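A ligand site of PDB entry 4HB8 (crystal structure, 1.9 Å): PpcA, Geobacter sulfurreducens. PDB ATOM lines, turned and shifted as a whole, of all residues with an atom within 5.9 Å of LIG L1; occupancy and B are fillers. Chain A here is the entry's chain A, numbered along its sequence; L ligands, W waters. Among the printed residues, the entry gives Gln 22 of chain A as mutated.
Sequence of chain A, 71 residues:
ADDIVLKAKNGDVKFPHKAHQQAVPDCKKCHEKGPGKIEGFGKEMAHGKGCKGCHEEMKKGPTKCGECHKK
SG of Cys 30 is bonded to C25 of LIG L1, at 2.0 Å. A ring nitrogen (NE2) of His 31 is bound to an iron atom (FE1) of LIG L1 (2.0 Å). SG of Cys 27 is covalently linked to C18 of LIG L1, at 2.0 Å. A ring nitrogen (NE2) of His 17 binds an iron atom (FE1) of LIG L1, at 2.0 Å. An oxygen (O2) of LIG L1 sits at hydrogen-bond distance from the backbone NH (N) of Ala 1 (2.6 Å). An iron atom (FE1) of LG2 L2 is bound by a ring nitrogen (NE2) of His 20, 2.0 Å away.
The side-chain amide nitrogen (NE2) of Gln 21 lies close to a ring nitrogen (ND1) of His 17 (3.3 Å). The side-chain carboxylate of Asp 3 sits at hydrogen-bond distance from the backbone NH of His 17, 3.0 Å away. O of Ile 4 is in hydrogen-bond range of N of Phe 15, at 3.0 Å. A ring nitrogen (ND1) of His 20 sits at hydrogen-bond distance from the backbone carbonyl oxygen of Pro 16 (2.7 Å).
The backbone carbonyl oxygen (O) of Asp 2 sits close to an oxygen (O3) of LIG L1. CA of Asp 3 touches O4 of LIG L1, 3.6 Å away. Ile 4 touches LIG L1. Phe 15 touches LIG L1 (CE2 to C31, 3.5 Å). CD2 of His 20 touches C26 of LIG L1, at 3.8 Å. Gln 21 touches LIG L1. Val 24 touches LIG L1 (CG1 to C24, 3.4 Å). CA of Pro 25 touches C19 of LIG L1 (3.99 Å). Hydrophobic or aromatic side chains that line LIG L1: Ala 1, Ile 4, Phe 15, His 17, His 20, Val 24 and His 31. 13 residues have an atom within 4 Å of LIG L1: Ala 1, Asp 2, Asp 3, Ile 4, Phe 15, His 17, His 20, Gln 21, Val 24, Pro 25, Cys 27, Cys 30 and His 31.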
ATOM      1  N   ALA A   1       2.537 -16.029  -9.392  1.00  0.00           N
ATOM      2  CA  ALA A   1       2.653 -14.925  -8.394  1.00  0.00           C
ATOM      3  C   ALA A   1       1.274 -14.355  -8.115  1.00  0.00           C
ATOM      4  O   ALA A   1       0.319 -14.604  -8.843  1.00  0.00           O
ATOM      5  CB  ALA A   1       3.593 -13.830  -8.900  1.00  0.00           C
ATOM      6  N   ASP A   2       1.193 -13.550  -7.073  1.00  0.00           N
ATOM      7  CA  ASP A   2      -0.069 -13.062  -6.597  1.00  0.00           C
ATOM      8  C   ASP A   2      -0.313 -11.641  -7.023  1.00  0.00           C
ATOM      9  O   ASP A   2       0.629 -10.923  -7.334  1.00  0.00           O
ATOM     10  CB  ASP A   2      -0.065 -13.124  -5.083  1.00  0.00           C
ATOM     11  CG  ASP A   2      -0.014 -14.524  -4.594  1.00  0.00           C
ATOM     12  OD1 ASP A   2      -0.920 -15.314  -5.007  1.00  0.00           O
ATOM     13  OD2 ASP A   2       0.885 -14.910  -3.797  1.00  0.00           O
ATOM     14  N   ASP A   3      -1.580 -11.259  -7.040  1.00  0.00           N
ATOM     15  CA  ASP A   3      -1.953  -9.852  -7.224  1.00  0.00           C
ATOM     16  C   ASP A   3      -1.436  -9.056  -6.064  1.00  0.00           C
ATOM     17  O   ASP A   3      -1.096  -9.600  -5.034  1.00  0.00           O
ATOM     18  CB  ASP A   3      -3.460  -9.695  -7.341  1.00  0.00           C
ATOM     19  CG  ASP A   3      -3.994 -10.236  -8.652  1.00  0.00           C
ATOM     20  OD1 ASP A   3      -3.195 -10.473  -9.584  1.00  0.00           O
ATOM     21  OD2 ASP A   3      -5.191 -10.433  -8.837  1.00  0.00           O
ATOM     22  N   ILE A   4      -1.325  -7.747  -6.263  1.00  0.00           N
ATOM     23  CA  ILE A   4      -0.898  -6.913  -5.168  1.00  0.00           C
ATOM     24  C   ILE A   4      -1.956  -5.850  -4.865  1.00  0.00           C
ATOM     25  O   ILE A   4      -2.799  -5.555  -5.704  1.00  0.00           O
ATOM     26  CB  ILE A   4       0.519  -6.299  -5.460  1.00  0.00           C
ATOM     27  CG1 ILE A   4       0.439  -4.879  -6.002  1.00  0.00           C
ATOM     28  CG2 ILE A   4       1.321  -7.149  -6.413  1.00  0.00           C
ATOM     29  CD1 ILE A   4       0.566  -3.840  -4.938  1.00  0.00           C
ATOM     30  N   PHE A  15      -4.828  -4.459  -7.696  1.00  0.00           N
ATOM     31  CA  PHE A  15      -4.296  -4.510  -9.045  1.00  0.00           C
ATOM     32  C   PHE A  15      -4.378  -5.961  -9.517  1.00  0.00           C
ATOM     33  O   PHE A  15      -3.561  -6.789  -9.092  1.00  0.00           O
ATOM     34  CB  PHE A  15      -2.825  -4.068  -9.092  1.00  0.00           C
ATOM     35  CG  PHE A  15      -2.238  -4.248 -10.459  1.00  0.00           C
ATOM     36  CD1 PHE A  15      -2.614  -3.386 -11.473  1.00  0.00           C
ATOM     37  CD2 PHE A  15      -1.431  -5.352 -10.746  1.00  0.00           C
ATOM     38  CE1 PHE A  15      -2.137  -3.569 -12.772  1.00  0.00           C
ATOM     39  CE2 PHE A  15      -0.952  -5.543 -12.034  1.00  0.00           C
ATOM     40  CZ  PHE A  15      -1.301  -4.659 -13.044  1.00  0.00           C
ATOM     41  N   PRO A  16      -5.385  -6.298 -10.313  1.00  0.00           N
ATOM     42  CA  PRO A  16      -5.512  -7.663 -10.819  1.00  0.00           C
ATOM     43  C   PRO A  16      -4.697  -7.889 -12.094  1.00  0.00           C
ATOM     44  O   PRO A  16      -5.016  -7.326 -13.141  1.00  0.00           O
ATOM     45  CB  PRO A  16      -7.013  -7.786 -11.080  1.00  0.00           C
ATOM     46  CG  PRO A  16      -7.443  -6.398 -11.468  1.00  0.00           C
ATOM     47  CD  PRO A  16      -6.507  -5.440 -10.750  1.00  0.00           C
ATOM     48  N   HIS A  17      -3.677  -8.739 -12.031  1.00  0.00           N
ATOM     49  CA  HIS A  17      -2.795  -8.876 -13.186  1.00  0.00           C
ATOM     50  C   HIS A  17      -3.463  -9.532 -14.403  1.00  0.00           C
ATOM     51  O   HIS A  17      -3.245  -9.084 -15.538  1.00  0.00           O
ATOM     52  CB  HIS A  17      -1.515  -9.657 -12.866  1.00  0.00           C
ATOM     53  CG  HIS A  17      -0.541  -9.632 -14.009  1.00  0.00           C
ATOM     54  ND1 HIS A  17      -0.380 -10.699 -14.861  1.00  0.00           N
ATOM     55  CD2 HIS A  17       0.266  -8.651 -14.475  1.00  0.00           C
ATOM     56  CE1 HIS A  17       0.513 -10.388 -15.781  1.00  0.00           C
ATOM     57  NE2 HIS A  17       0.934  -9.156 -15.565  1.00  0.00           N
ATOM     58  N   HIS A  20      -5.202  -7.408 -16.809  1.00  0.00           N
ATOM     59  CA  HIS A  20      -4.243  -6.580 -17.550  1.00  0.00           C
ATOM     60  C   HIS A  20      -3.477  -7.343 -18.637  1.00  0.00           C
ATOM     61  O   HIS A  20      -3.268  -6.822 -19.732  1.00  0.00           O
ATOM     62  CB  HIS A  20      -3.298  -5.892 -16.583  1.00  0.00           C
ATOM     63  CG  HIS A  20      -3.989  -4.824 -15.803  1.00  0.00           C
ATOM     64  ND1 HIS A  20      -4.697  -5.095 -14.656  1.00  0.00           N
ATOM     65  CD2 HIS A  20      -4.187  -3.508 -16.065  1.00  0.00           C
ATOM     66  CE1 HIS A  20      -5.252  -3.986 -14.215  1.00  0.00           C
ATOM     67  NE2 HIS A  20      -4.955  -3.000 -15.048  1.00  0.00           N
ATOM     68  N   GLN A  21      -3.035  -8.548 -18.327  1.00  0.00           N
ATOM     69  CA  GLN A  21      -2.352  -9.388 -19.308  1.00  0.00           C
ATOM     70  C   GLN A  21      -3.268  -9.641 -20.520  1.00  0.00           C
ATOM     71  O   GLN A  21      -2.799  -9.638 -21.666  1.00  0.00           O
ATOM     72  CB  GLN A  21      -1.934 -10.704 -18.666  1.00  0.00           C
ATOM     73  CG  GLN A  21      -1.046 -11.575 -19.523  1.00  0.00           C
ATOM     74  CD  GLN A  21      -0.437 -12.765 -18.759  1.00  0.00           C
ATOM     75  OE1 GLN A  21       0.014 -13.715 -19.376  1.00  0.00           O
ATOM     76  NE2 GLN A  21      -0.432 -12.706 -17.449  1.00  0.00           N
ATOM     77  N   GLN A  22      -4.562  -9.815 -20.250  1.00  0.00           N
ATOM     78  CA  GLN A  22      -5.549 -10.088 -21.296  1.00  0.00           C
ATOM     79  C   GLN A  22      -5.917  -8.839 -22.104  1.00  0.00           C
ATOM     80  O   GLN A  22      -5.890  -8.862 -23.346  1.00  0.00           O
ATOM     81  CB  GLN A  22      -6.777 -10.786 -20.710  1.00  0.00           C
ATOM     82  CG  GLN A  22      -6.459 -12.212 -20.255  1.00  0.00           C
ATOM     83  CD  GLN A  22      -7.653 -12.965 -19.663  1.00  0.00           C
ATOM     84  OE1 GLN A  22      -7.537 -14.145 -19.346  1.00  0.00           O
ATOM     85  NE2 GLN A  22      -8.779 -12.280 -19.514  1.00  0.00           N
ATOM     86  N   VAL A  24      -4.236  -5.843 -22.199  1.00  0.00           N
ATOM     87  CA  VAL A  24      -3.114  -4.993 -22.589  1.00  0.00           C
ATOM     88  C   VAL A  24      -1.998  -5.903 -23.143  1.00  0.00           C
ATOM     89  O   VAL A  24      -0.954  -6.074 -22.535  1.00  0.00           O
ATOM     90  CB  VAL A  24      -2.592  -4.106 -21.414  1.00  0.00           C
ATOM     91  CG1 VAL A  24      -1.540  -3.136 -21.882  1.00  0.00           C
ATOM     92  CG2 VAL A  24      -3.739  -3.341 -20.753  1.00  0.00           C
ATOM     93  N   PRO A  25      -2.260  -6.494 -24.309  1.00  0.00           N
ATOM     94  CA  PRO A  25      -1.248  -7.370 -24.956  1.00  0.00           C
ATOM     95  C   PRO A  25       0.078  -6.684 -25.296  1.00  0.00           C
ATOM     96  O   PRO A  25       1.094  -7.363 -25.495  1.00  0.00           O
ATOM     97  CB  PRO A  25      -1.984  -7.876 -26.209  1.00  0.00           C
ATOM     98  CG  PRO A  25      -3.046  -6.865 -26.476  1.00  0.00           C
ATOM     99  CD  PRO A  25      -3.514  -6.417 -25.074  1.00  0.00           C
ATOM    100  N   ASP A  26       0.087  -5.363 -25.379  1.00  0.00           N
ATOM    101  CA  ASP A  26       1.322  -4.622 -25.439  1.00  0.00           C
ATOM    102  C   ASP A  26       1.946  -4.567 -24.029  1.00  0.00           C
ATOM    103  O   ASP A  26       1.811  -3.581 -23.298  1.00  0.00           O
ATOM    104  CB  ASP A  26       1.078  -3.231 -26.014  1.00  0.00           C
ATOM    105  CG  ASP A  26       2.345  -2.471 -26.297  1.00  0.00           C
ATOM    106  OD1 ASP A  26       3.469  -2.944 -26.005  1.00  0.00           O
ATOM    107  OD2 ASP A  26       2.304  -1.327 -26.787  1.00  0.00           O
ATOM    108  N   CYS A  27       2.655  -5.637 -23.674  1.00  0.00           N
ATOM    109  CA  CYS A  27       3.264  -5.822 -22.347  1.00  0.00           C
ATOM    110  C   CYS A  27       4.271  -4.754 -22.040  1.00  0.00           C
ATOM    111  O   CYS A  27       4.479  -4.432 -20.874  1.00  0.00           O
ATOM    112  CB  CYS A  27       3.952  -7.181 -22.246  1.00  0.00           C
ATOM    113  SG  CYS A  27       3.027  -8.594 -22.874  1.00  0.00           S
ATOM    114  N   LYS A  29       3.979  -1.739 -22.270  1.00  0.00           N
ATOM    115  CA  LYS A  29       3.344  -0.625 -21.535  1.00  0.00           C
ATOM    116  C   LYS A  29       3.770  -0.583 -20.087  1.00  0.00           C
ATOM    117  O   LYS A  29       3.872   0.488 -19.488  1.00  0.00           O
ATOM    118  CB  LYS A  29       1.833  -0.696 -21.664  1.00  0.00           C
ATOM    119  CG  LYS A  29       1.343  -0.316 -23.040  1.00  0.00           C
ATOM    120  CD  LYS A  29       1.639   1.156 -23.293  1.00  0.00           C
ATOM    121  N   CYS A  30       4.052  -1.749 -19.516  1.00  0.00           N
ATOM    122  CA  CYS A  30       4.450  -1.852 -18.121  1.00  0.00           C
ATOM    123  C   CYS A  30       5.770  -2.549 -17.868  1.00  0.00           C
ATOM    124  O   CYS A  30       6.420  -2.257 -16.873  1.00  0.00           O
ATOM    125  CB  CYS A  30       3.376  -2.629 -17.395  1.00  0.00           C
ATOM    126  SG  CYS A  30       1.800  -1.750 -17.334  1.00  0.00           S
ATOM    127  N   HIS A  31       6.121  -3.512 -18.705  1.00  0.00           N
ATOM    128  CA  HIS A  31       7.313  -4.326 -18.496  1.00  0.00           C
ATOM    129  C   HIS A  31       8.481  -3.875 -19.405  1.00  0.00           C
ATOM    130  O   HIS A  31       8.285  -3.203 -20.404  1.00  0.00           O
ATOM    131  CB  HIS A  31       6.988  -5.807 -18.721  1.00  0.00           C
ATOM    132  CG  HIS A  31       6.038  -6.379 -17.704  1.00  0.00           C
ATOM    133  ND1 HIS A  31       6.290  -6.373 -16.347  1.00  0.00           N
ATOM    134  CD2 HIS A  31       4.818  -6.956 -17.844  1.00  0.00           C
ATOM    135  CE1 HIS A  31       5.283  -6.941 -15.704  1.00  0.00           C
ATOM    136  NE2 HIS A  31       4.370  -7.296 -16.582  1.00  0.00           N
ATOM    137  N   GLY A  50       0.164   5.973 -14.962  1.00  0.00           N
ATOM    138  CA  GLY A  50       0.353   4.744 -14.183  1.00  0.00           C
ATOM    139  C   GLY A  50      -0.860   3.866 -14.007  1.00  0.00           C
ATOM    140  O   GLY A  50      -0.747   2.644 -13.956  1.00  0.00           O
HETATM  141 FE1  LIG L   1       2.675  -8.246 -16.128  1.00  0.00          FE
HETATM  142  C1  LIG L   1       3.572  -9.632 -13.127  1.00  0.00           C
HETATM  143  C2  LIG L   1       3.979 -10.861 -17.775  1.00  0.00           C
HETATM  144  C3  LIG L   1       1.072  -7.173 -18.992  1.00  0.00           C
HETATM  145  C4  LIG L   1       2.123  -5.268 -14.641  1.00  0.00           C
HETATM  146  N1  LIG L   1       3.667  -9.845 -15.567  1.00  0.00           N
HETATM  147  C5  LIG L   1       3.798 -10.338 -14.286  1.00  0.00           C
HETATM  148  C6  LIG L   1       4.216 -11.708 -14.350  1.00  0.00           C
HETATM  149  C7  LIG L   1       4.343 -12.056 -15.623  1.00  0.00           C
HETATM  150  C8  LIG L   1       4.002 -10.907 -16.422  1.00  0.00           C
HETATM  151  C9  LIG L   1       4.777 -13.436 -16.190  1.00  0.00           C
HETATM  152  C10 LIG L   1       4.405 -12.612 -13.124  1.00  0.00           C
HETATM  153  C11 LIG L   1       2.985 -13.195 -12.906  1.00  0.00           C
HETATM  154  C12 LIG L   1       2.937 -14.481 -12.099  1.00  0.00           C
HETATM  155  O1  LIG L   1       3.969 -15.186 -11.890  1.00  0.00           O
HETATM  156  O2  LIG L   1       1.803 -14.807 -11.620  1.00  0.00           O
HETATM  157  N2  LIG L   1       2.526  -8.896 -18.058  1.00  0.00           N
HETATM  158  C13 LIG L   1       3.169 -10.032 -18.523  1.00  0.00           C
HETATM  159  C14 LIG L   1       2.882 -10.168 -19.939  1.00  0.00           C
HETATM  160  C15 LIG L   1       2.067  -9.143 -20.286  1.00  0.00           C
HETATM  161  C16 LIG L   1       1.835  -8.328 -19.087  1.00  0.00           C
HETATM  162  C17 LIG L   1       3.460 -11.310 -20.813  1.00  0.00           C
HETATM  163  C18 LIG L   1       1.428  -8.782 -21.653  1.00  0.00           C
HETATM  164  C19 LIG L   1       0.511  -9.609 -22.165  1.00  0.00           C
HETATM  165  N3  LIG L   1       1.761  -6.566 -16.712  1.00  0.00           N
HETATM  166  C20 LIG L   1       1.175  -6.277 -17.945  1.00  0.00           C
HETATM  167  C21 LIG L   1       0.729  -4.896 -17.922  1.00  0.00           C
HETATM  168  C22 LIG L   1       1.014  -4.402 -16.716  1.00  0.00           C
HETATM  169  C23 LIG L   1       1.685  -5.424 -15.942  1.00  0.00           C
HETATM  170  C24 LIG L   1       0.040  -4.137 -19.084  1.00  0.00           C
HETATM  171  C25 LIG L   1       0.740  -2.967 -16.203  1.00  0.00           C
HETATM  172  C26 LIG L   1      -0.545  -2.485 -16.330  1.00  0.00           C
HETATM  173  N4  LIG L   1       2.861  -7.537 -14.186  1.00  0.00           N
HETATM  174  C27 LIG L   1       2.554  -6.271 -13.816  1.00  0.00           C
HETATM  175  C28 LIG L   1       2.704  -6.160 -12.390  1.00  0.00           C
HETATM  176  C29 LIG L   1       3.164  -7.517 -11.894  1.00  0.00           C
HETATM  177  C30 LIG L   1       3.237  -8.315 -13.099  1.00  0.00           C
HETATM  178  C31 LIG L   1       2.484  -4.907 -11.566  1.00  0.00           C
HETATM  179  C32 LIG L   1       3.455  -7.949 -10.456  1.00  0.00           C
HETATM  180  C33 LIG L   1       2.157  -7.866  -9.647  1.00  0.00           C
HETATM  181  C34 LIG L   1       1.126  -8.893 -10.062  1.00  0.00           C
HETATM  182  O3  LIG L   1       1.494 -10.022 -10.463  1.00  0.00           O
HETATM  183  O4  LIG L   1      -0.069  -8.531  -9.944  1.00  0.00           O
HETATM  184 FE1  LG2 L   2      -5.923  -1.216 -15.220  1.00  0.00          FE
HETATM  185  C1  LG2 L   2      -8.824  -2.928 -15.858  1.00  0.00           C
HETATM  186  C2  LG2 L   2      -6.678  -1.254 -11.859  1.00  0.00           C
HETATM  187  C3  LG2 L   2      -2.938   0.264 -14.513  1.00  0.00           C
HETATM  188  C4  LG2 L   2      -5.281  -0.891 -18.542  1.00  0.00           C
HETATM  189  N1  LG2 L   2      -7.473  -1.933 -14.080  1.00  0.00           N
HETATM  190  C5  LG2 L   2      -8.556  -2.658 -14.534  1.00  0.00           C
HETATM  191  C6  LG2 L   2      -9.324  -3.120 -13.389  1.00  0.00           C
HETATM  192  C7  LG2 L   2      -8.738  -2.654 -12.287  1.00  0.00           C
HETATM  193  C8  LG2 L   2      -7.564  -1.892 -12.689  1.00  0.00           C
HETATM  194  C9  LG2 L   2      -9.203  -2.876 -10.843  1.00  0.00           C
HETATM  195  C10 LG2 L   2     -10.627  -3.955 -13.463  1.00  0.00           C
HETATM  196  C11 LG2 L   2     -10.363  -5.367 -13.939  1.00  0.00           C
HETATM  197  C12 LG2 L   2     -11.675  -6.087 -14.130  1.00  0.00           C
HETATM  198  O1  LG2 L   2     -12.665  -5.460 -14.539  1.00  0.00           O
HETATM  199  O2  LG2 L   2     -11.721  -7.309 -13.848  1.00  0.00           O
HETATM  200  N2  LG2 L   2      -4.994  -0.619 -13.531  1.00  0.00           N
HETATM  201  C13 LG2 L   2      -5.473  -0.705 -12.250  1.00  0.00           C
HETATM  202  C14 LG2 L   2      -4.504  -0.104 -11.363  1.00  0.00           C
HETATM  203  C15 LG2 L   2      -3.478   0.290 -12.087  1.00  0.00           C
HETATM  204  C16 LG2 L   2      -3.764  -0.031 -13.465  1.00  0.00           C
HETATM  205  C17 LG2 L   2      -4.682  -0.002  -9.839  1.00  0.00           C
HETATM  206  C18 LG2 L   2      -2.174   0.940 -11.644  1.00  0.00           C
HETATM  207  C19 LG2 L   2      -1.527   0.358 -10.591  1.00  0.00           C
HETATM  208  N3  LG2 L   2      -4.399  -0.427 -16.319  1.00  0.00           N
HETATM  209  C20 LG2 L   2      -3.250   0.112 -15.829  1.00  0.00           C
HETATM  210  C21 LG2 L   2      -2.406   0.467 -16.942  1.00  0.00           C
HETATM  211  C22 LG2 L   2      -3.030   0.133 -18.082  1.00  0.00           C
HETATM  212  C23 LG2 L   2      -4.312  -0.412 -17.703  1.00  0.00           C
HETATM  213  C24 LG2 L   2      -1.026   1.115 -16.763  1.00  0.00           C
HETATM  214  C25 LG2 L   2      -2.551   0.315 -19.540  1.00  0.00           C
HETATM  215  C26 LG2 L   2      -1.269   0.540 -19.824  1.00  0.00           C
HETATM  216  N4  LG2 L   2      -6.875  -1.833 -16.930  1.00  0.00           N
HETATM  217  C27 LG2 L   2      -6.450  -1.514 -18.213  1.00  0.00           C
HETATM  218  C28 LG2 L   2      -7.445  -1.957 -19.173  1.00  0.00           C
HETATM  219  C29 LG2 L   2      -8.526  -2.595 -18.313  1.00  0.00           C
HETATM  220  C30 LG2 L   2      -8.097  -2.464 -16.941  1.00  0.00           C
HETATM  221  C31 LG2 L   2      -7.466  -1.858 -20.709  1.00  0.00           C
HETATM  222  C32 LG2 L   2      -9.835  -3.258 -18.766  1.00  0.00           C
HETATM  223  C33 LG2 L   2      -9.693  -4.743 -18.507  1.00  0.00           C
HETATM  224  C34 LG2 L   2     -11.029  -5.439 -18.622  1.00  0.00           C
HETATM  225  O3  LG2 L   2     -12.048  -4.895 -18.113  1.00  0.00           O
HETATM  226  O4  LG2 L   2     -11.064  -6.535 -19.214  1.00  0.00           O
HETATM  227  C1  LG3 L   3       4.850   0.204  -6.251  1.00  0.00           C
HETATM  228  C2  LG3 L   3       3.572  -0.082  -7.047  1.00  0.00           C
HETATM  229  C3  LG3 L   3       3.692  -1.434  -7.778  1.00  0.00           C
HETATM  230  C4  LG3 L   3       4.885  -1.493  -8.759  1.00  0.00           C
HETATM  231  C5  LG3 L   3       6.156  -1.129  -7.965  1.00  0.00           C
HETATM  232  C6  LG3 L   3       6.027   0.206  -7.226  1.00  0.00           C
HETATM  233  C7  LG3 L   3       2.347  -1.776  -8.454  1.00  0.00           C
HETATM  234  C8  LG3 L   3       2.103  -0.898  -9.728  1.00  0.00           C
HETATM  235  C9  LG3 L   3       3.295  -0.924 -10.692  1.00  0.00           C
HETATM  236  C10 LG3 L   3       4.633  -0.596  -9.971  1.00  0.00           C
HETATM  237  C11 LG3 L   3       3.127   0.072 -11.851  1.00  0.00           C
HETATM  238  C12 LG3 L   3       4.232  -0.056 -12.906  1.00  0.00           C
HETATM  239  C13 LG3 L   3       5.570   0.287 -12.237  1.00  0.00           C
HETATM  240  C14 LG3 L   3       5.807  -0.615 -10.999  1.00  0.00           C
HETATM  241  C15 LG3 L   3       1.816  -0.069 -12.674  1.00  0.00           C
HETATM  242  C16 LG3 L   3       2.194   0.515 -14.043  1.00  0.00           C
HETATM  243  C17 LG3 L   3       3.679   0.958 -13.929  1.00  0.00           C
HETATM  244  C18 LG3 L   3       5.063  -2.965  -9.205  1.00  0.00           C
HETATM  245  C19 LG3 L   3       4.367   0.946 -15.318  1.00  0.00           C
HETATM  246  O1  LG3 L   3       5.629   1.679 -11.816  1.00  0.00           O
HETATM  247  O2  LG3 L   3       4.804   1.514  -5.652  1.00  0.00           O
HETATM  248  C20 LG3 L   3       4.273  -1.458 -13.520  1.00  0.00           C
HETATM  249  C21 LG3 L   3       3.572   1.798 -16.329  1.00  0.00           C
HETATM  250  C22 LG3 L   3       3.461   3.265 -15.915  1.00  0.00           C
HETATM  251  C23 LG3 L   3       4.576   4.113 -16.512  1.00  0.00           C
HETATM  252  O3  LG3 L   3       4.727   4.161 -17.736  1.00  0.00           O
HETATM  253  O4  LG3 L   3       5.320   4.766 -15.757  1.00  0.00           O
HETATM  254  C24 LG3 L   3       5.828   1.402 -15.262  1.00  0.00           C
HETATM  255  O   HOH W   1      -0.531 -11.648 -10.315  1.00  0.00           O
